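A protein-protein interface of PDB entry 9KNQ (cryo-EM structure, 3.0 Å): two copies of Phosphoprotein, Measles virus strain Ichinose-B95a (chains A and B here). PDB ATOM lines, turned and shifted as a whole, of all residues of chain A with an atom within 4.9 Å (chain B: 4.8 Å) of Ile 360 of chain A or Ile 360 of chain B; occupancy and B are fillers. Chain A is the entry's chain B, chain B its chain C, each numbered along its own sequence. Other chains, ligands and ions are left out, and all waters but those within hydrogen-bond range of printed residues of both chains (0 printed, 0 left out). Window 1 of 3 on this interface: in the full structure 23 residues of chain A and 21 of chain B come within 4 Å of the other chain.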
ATOM      1  N   GLN A 356       7.849 -25.126 -10.628  1.00  0.00           N
ATOM      2  CA  GLN A 356       6.873 -24.258 -11.276  1.00  0.00           C
ATOM      3  C   GLN A 356       7.427 -23.683 -12.573  1.00  0.00           C
ATOM      4  O   GLN A 356       6.701 -23.565 -13.568  1.00  0.00           O
ATOM      5  CB  GLN A 356       6.456 -23.139 -10.326  1.00  0.00           C
ATOM      6  CG  GLN A 356       5.517 -22.123 -10.941  1.00  0.00           C
ATOM      7  CD  GLN A 356       5.326 -20.912 -10.058  1.00  0.00           C
ATOM      8  OE1 GLN A 356       5.797 -19.819 -10.372  1.00  0.00           O
ATOM      9  NE2 GLN A 356       4.639 -21.100  -8.938  1.00  0.00           N
ATOM     10  N   ASN A 357       8.714 -23.332 -12.589  1.00  0.00           N
ATOM     11  CA  ASN A 357       9.274 -22.733 -13.796  1.00  0.00           C
ATOM     12  C   ASN A 357       9.341 -23.740 -14.942  1.00  0.00           C
ATOM     13  O   ASN A 357       9.120 -23.380 -16.104  1.00  0.00           O
ATOM     14  CB  ASN A 357      10.646 -22.115 -13.502  1.00  0.00           C
ATOM     15  CG  ASN A 357      11.798 -23.075 -13.734  1.00  0.00           C
ATOM     16  OD1 ASN A 357      11.674 -24.281 -13.542  1.00  0.00           O
ATOM     17  ND2 ASN A 357      12.933 -22.535 -14.165  1.00  0.00           N
ATOM     18  N   ILE A 358       9.616 -25.015 -14.645  1.00  0.00           N
ATOM     19  CA  ILE A 358       9.644 -25.983 -15.737  1.00  0.00           C
ATOM     20  C   ILE A 358       8.228 -26.315 -16.191  1.00  0.00           C
ATOM     21  O   ILE A 358       8.007 -26.607 -17.373  1.00  0.00           O
ATOM     22  CB  ILE A 358      10.465 -27.243 -15.370  1.00  0.00           C
ATOM     23  CG1 ILE A 358       9.977 -27.955 -14.097  1.00  0.00           C
ATOM     24  CG2 ILE A 358      11.953 -26.909 -15.292  1.00  0.00           C
ATOM     25  CD1 ILE A 358       8.751 -28.852 -14.261  1.00  0.00           C
ATOM     26  N   SER A 359       7.245 -26.252 -15.289  1.00  0.00           N
ATOM     27  CA  SER A 359       5.860 -26.356 -15.742  1.00  0.00           C
ATOM     28  C   SER A 359       5.519 -25.222 -16.705  1.00  0.00           C
ATOM     29  O   SER A 359       4.875 -25.441 -17.743  1.00  0.00           O
ATOM     30  CB  SER A 359       4.911 -26.361 -14.545  1.00  0.00           C
ATOM     31  OG  SER A 359       4.312 -25.094 -14.362  1.00  0.00           O
ATOM     32  N   ILE A 360       5.959 -24.003 -16.379  1.00  0.00           N
ATOM     33  CA  ILE A 360       5.789 -22.869 -17.289  1.00  0.00           C
ATOM     34  C   ILE A 360       6.436 -23.168 -18.635  1.00  0.00           C
ATOM     35  O   ILE A 360       5.863 -22.890 -19.695  1.00  0.00           O
ATOM     36  CB  ILE A 360       6.379 -21.585 -16.678  1.00  0.00           C
ATOM     37  CG1 ILE A 360       5.423 -20.983 -15.652  1.00  0.00           C
ATOM     38  CG2 ILE A 360       6.651 -20.566 -17.765  1.00  0.00           C
ATOM     39  CD1 ILE A 360       5.850 -19.634 -15.135  1.00  0.00           C
ATOM     40  N   SER A 361       7.652 -23.719 -18.608  1.00  0.00           N
ATOM     41  CA  SER A 361       8.383 -23.968 -19.846  1.00  0.00           C
ATOM     42  C   SER A 361       7.673 -24.998 -20.713  1.00  0.00           C
ATOM     43  O   SER A 361       7.630 -24.858 -21.939  1.00  0.00           O
ATOM     44  CB  SER A 361       9.806 -24.426 -19.532  1.00  0.00           C
ATOM     45  OG  SER A 361      10.295 -25.281 -20.550  1.00  0.00           O
ATOM     46  N   THR A 362       7.117 -26.046 -20.101  1.00  0.00           N
ATOM     47  CA  THR A 362       6.380 -27.023 -20.899  1.00  0.00           C
ATOM     48  C   THR A 362       5.104 -26.417 -21.468  1.00  0.00           C
ATOM     49  O   THR A 362       4.731 -26.709 -22.610  1.00  0.00           O
ATOM     50  CB  THR A 362       6.061 -28.279 -20.090  1.00  0.00           C
ATOM     51  OG1 THR A 362       4.990 -28.017 -19.174  1.00  0.00           O
ATOM     52  CG2 THR A 362       7.286 -28.783 -19.354  1.00  0.00           C
ATOM     53  N   LEU A 363       4.421 -25.565 -20.695  1.00  0.00           N
ATOM     54  CA  LEU A 363       3.251 -24.884 -21.248  1.00  0.00           C
ATOM     55  C   LEU A 363       3.633 -24.021 -22.446  1.00  0.00           C
ATOM     56  O   LEU A 363       2.924 -23.998 -23.462  1.00  0.00           O
ATOM     57  CB  LEU A 363       2.567 -24.037 -20.177  1.00  0.00           C
ATOM     58  CG  LEU A 363       1.393 -23.182 -20.665  1.00  0.00           C
ATOM     59  CD1 LEU A 363       0.178 -23.368 -19.775  1.00  0.00           C
ATOM     60  CD2 LEU A 363       1.772 -21.713 -20.731  1.00  0.00           C
ATOM     61  N   GLU A 364       4.752 -23.303 -22.342  1.00  0.00           N
ATOM     62  CA  GLU A 364       5.203 -22.457 -23.443  1.00  0.00           C
ATOM     63  C   GLU A 364       5.553 -23.295 -24.665  1.00  0.00           C
ATOM     64  O   GLU A 364       5.200 -22.942 -25.795  1.00  0.00           O
ATOM     65  CB  GLU A 364       6.402 -21.616 -23.006  1.00  0.00           C
ATOM     66  CG  GLU A 364       6.917 -20.656 -24.073  1.00  0.00           C
ATOM     67  CD  GLU A 364       7.973 -21.279 -24.965  1.00  0.00           C
ATOM     68  OE1 GLU A 364       8.343 -20.660 -25.985  1.00  0.00           O
ATOM     69  OE2 GLU A 364       8.434 -22.394 -24.647  1.00  0.00           O
ATOM     70  N   GLN B 356       0.285 -18.463  -7.722  1.00  0.00           N
ATOM     71  CA  GLN B 356       0.864 -18.687  -9.046  1.00  0.00           C
ATOM     72  C   GLN B 356       0.565 -20.096  -9.551  1.00  0.00           C
ATOM     73  O   GLN B 356       0.266 -20.291 -10.738  1.00  0.00           O
ATOM     74  CB  GLN B 356       2.371 -18.432  -9.025  1.00  0.00           C
ATOM     75  CG  GLN B 356       2.744 -16.960  -9.078  1.00  0.00           C
ATOM     76  CD  GLN B 356       4.116 -16.723  -9.672  1.00  0.00           C
ATOM     77  OE1 GLN B 356       4.566 -15.582  -9.790  1.00  0.00           O
ATOM     78  NE2 GLN B 356       4.789 -17.799 -10.055  1.00  0.00           N
ATOM     79  N   ASN B 357       0.625 -21.089  -8.661  1.00  0.00           N
ATOM     80  CA  ASN B 357       0.364 -22.467  -9.065  1.00  0.00           C
ATOM     81  C   ASN B 357      -1.091 -22.654  -9.478  1.00  0.00           C
ATOM     82  O   ASN B 357      -1.384 -23.289 -10.499  1.00  0.00           O
ATOM     83  CB  ASN B 357       0.726 -23.427  -7.933  1.00  0.00           C
ATOM     84  CG  ASN B 357       2.202 -23.751  -7.892  1.00  0.00           C
ATOM     85  OD1 ASN B 357       2.731 -24.146  -6.854  1.00  0.00           O
ATOM     86  ND2 ASN B 357       2.877 -23.590  -9.024  1.00  0.00           N
ATOM     87  N   ILE B 358      -2.022 -22.111  -8.689  1.00  0.00           N
ATOM     88  CA  ILE B 358      -3.427 -22.252  -9.038  1.00  0.00           C
ATOM     89  C   ILE B 358      -3.763 -21.458 -10.295  1.00  0.00           C
ATOM     90  O   ILE B 358      -4.724 -21.800 -10.996  1.00  0.00           O
ATOM     91  CB  ILE B 358      -4.332 -21.849  -7.854  1.00  0.00           C
ATOM     92  CG1 ILE B 358      -5.750 -22.390  -8.052  1.00  0.00           C
ATOM     93  CG2 ILE B 358      -4.384 -20.342  -7.689  1.00  0.00           C
ATOM     94  CD1 ILE B 358      -5.799 -23.841  -8.481  1.00  0.00           C
ATOM     95  N   SER B 359      -2.988 -20.419 -10.620  1.00  0.00           N
ATOM     96  CA  SER B 359      -3.249 -19.678 -11.849  1.00  0.00           C
ATOM     97  C   SER B 359      -2.656 -20.356 -13.078  1.00  0.00           C
ATOM     98  O   SER B 359      -3.195 -20.205 -14.180  1.00  0.00           O
ATOM     99  CB  SER B 359      -2.705 -18.256 -11.733  1.00  0.00           C
ATOM    100  OG  SER B 359      -1.499 -18.247 -11.007  1.00  0.00           O
ATOM    101  N   ILE B 360      -1.546 -21.081 -12.930  1.00  0.00           N
ATOM    102  CA  ILE B 360      -1.023 -21.821 -14.077  1.00  0.00           C
ATOM    103  C   ILE B 360      -1.777 -23.131 -14.296  1.00  0.00           C
ATOM    104  O   ILE B 360      -1.817 -23.642 -15.429  1.00  0.00           O
ATOM    105  CB  ILE B 360       0.488 -22.079 -13.933  1.00  0.00           C
ATOM    106  CG1 ILE B 360       1.014 -22.866 -15.136  1.00  0.00           C
ATOM    107  CG2 ILE B 360       0.792 -22.824 -12.652  1.00  0.00           C
ATOM    108  CD1 ILE B 360       2.475 -22.740 -15.350  1.00  0.00           C
ATOM    109  N   SER B 361      -2.383 -23.689 -13.244  1.00  0.00           N
ATOM    110  CA  SER B 361      -3.160 -24.912 -13.406  1.00  0.00           C
ATOM    111  C   SER B 361      -4.259 -24.730 -14.447  1.00  0.00           C
ATOM    112  O   SER B 361      -4.402 -25.547 -15.362  1.00  0.00           O
ATOM    113  CB  SER B 361      -3.756 -25.336 -12.064  1.00  0.00           C
ATOM    114  OG  SER B 361      -4.352 -26.617 -12.168  1.00  0.00           O
ATOM    115  N   THR B 362      -5.035 -23.651 -14.333  1.00  0.00           N
ATOM    116  CA  THR B 362      -6.120 -23.432 -15.283  1.00  0.00           C
ATOM    117  C   THR B 362      -5.597 -23.098 -16.674  1.00  0.00           C
ATOM    118  O   THR B 362      -6.249 -23.423 -17.672  1.00  0.00           O
ATOM    119  CB  THR B 362      -7.040 -22.325 -14.780  1.00  0.00           C
ATOM    120  OG1 THR B 362      -7.813 -21.803 -15.870  1.00  0.00           O
ATOM    121  CG2 THR B 362      -6.228 -21.218 -14.152  1.00  0.00           C
ATOM    122  N   LEU B 363      -4.432 -22.455 -16.763  1.00  0.00           N
ATOM    123  CA  LEU B 363      -3.815 -22.203 -18.061  1.00  0.00           C
ATOM    124  C   LEU B 363      -3.540 -23.511 -18.793  1.00  0.00           C
ATOM    125  O   LEU B 363      -3.976 -23.713 -19.936  1.00  0.00           O
ATOM    126  CB  LEU B 363      -2.523 -21.409 -17.875  1.00  0.00           C
ATOM    127  CG  LEU B 363      -2.106 -20.482 -19.017  1.00  0.00           C
ATOM    128  CD1 LEU B 363      -3.325 -19.875 -19.698  1.00  0.00           C
ATOM    129  CD2 LEU B 363      -1.163 -19.401 -18.510  1.00  0.00           C
ATOM    130  N   GLU B 364      -2.808 -24.418 -18.141  1.00  0.00           N
ATOM    131  CA  GLU B 364      -2.508 -25.692 -18.786  1.00  0.00           C
ATOM    132  C   GLU B 364      -3.764 -26.535 -18.973  1.00  0.00           C
ATOM    133  O   GLU B 364      -3.840 -27.325 -19.920  1.00  0.00           O
ATOM    134  CB  GLU B 364      -1.448 -26.458 -17.995  1.00  0.00           C
ATOM    135  CG  GLU B 364      -1.914 -26.995 -16.663  1.00  0.00           C
ATOM    136  CD  GLU B 364      -0.764 -27.464 -15.801  1.00  0.00           C
ATOM    137  OE1 GLU B 364      -0.895 -27.418 -14.560  1.00  0.00           O
ATOM    138  OE2 GLU B 364       0.272 -27.875 -16.361  1.00  0.00           O
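NE2 of Gln 356 of chain B sits close to NE2 of Gln 356 of chain A, 3.5 Å away.
The side-chain amide nitrogen of Asn 357 of chain B lies close to the side-chain amide nitrogen of Gln 356 of chain A.
The side-chain hydroxyl (OG) of Ser 359 of chain A sits at hydrogen-bond distance from the backbone carbonyl oxygen (O) of Gln 356 of chain A (2.9 Å).
O of Ser 359 of chain A sits at hydrogen-bond distance from OG1 of Thr 362 of chain A.
The side-chain hydroxyl of Ser 359 of chain B sits at hydrogen-bond distance from the backbone carbonyl oxygen of Gln 356 of chain B, at 2.7 Å.
Among the printed residues, pairs that only touch across the chains: Ser 359 of chain A with Ile 360 of chain B (3.1 Å), Ile 360 of chain A with Ile 360 of chain B (3.4 Å), Leu 363 of chain A with Leu 363 of chain B (3.8 Å) and Leu 363 of chain A with Glu 364 of chain B (3.6 Å).
Of the printed residues of chain B, Ile 360 of chain A touches Ile 360.
Printed residues of chain B within 4 Å of Ser 359 of chain A: Ile 360 (3.1 Å).
Printed residues of chain B within 4 Å of Gln 356 of chain A: Gln 356 (2.3 Å) and Asn 357 (3.1 Å).
Of the printed residues of chain B, Leu 363 of chain A touches Leu 363 and Glu 364.
The nearest residue of chain A that does not touch Ile 360 of chain B is Gln 356 of chain A (4.7 Å).
The nearest printed residue of chain A that does not touch Leu 363 of chain B is Ile 360 of chain A (7.4 Å).
Of the 9 printed residues of chain B, 5 touch a printed residue of chain A.
Of the 9 printed residues of chain A, 4 touch a printed residue of chain B.
Printed residues of chain A that touch a printed residue of chain B: Gln 356, Ser 359, Ile 360 and Leu 363.
Among the printed residues, 6 pairs touch across the chains.
Among the printed residues, no Asp or Glu carboxylate lies within 4 Å of a Lys or Arg side-chain nitrogen of the other chain.
Gln 356 of chain A touches Asn 357 of chain B, but with the chains exchanged Asn 357 of chain A does not touch Gln 356 of chain B (7.2 Å).
Ser 359 of chain A touches Ile 360 of chain B, but with the chains exchanged Ile 360 of chain A does not touch Ser 359 of chain B (8.5 Å).
Ile 360 of chain B touches its own counterpart, Ile 360 of chain A.
Leu 363 of chain A touches its own counterpart, Leu 363 of chain B.
Positions printed for both chains: 356, 357, 358, 359, 360, 361, 362, 363 and 364.
Of the 6 pairs that touch across the chains among the printed residues, 3 have their exchanged pair printed and touching as well.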
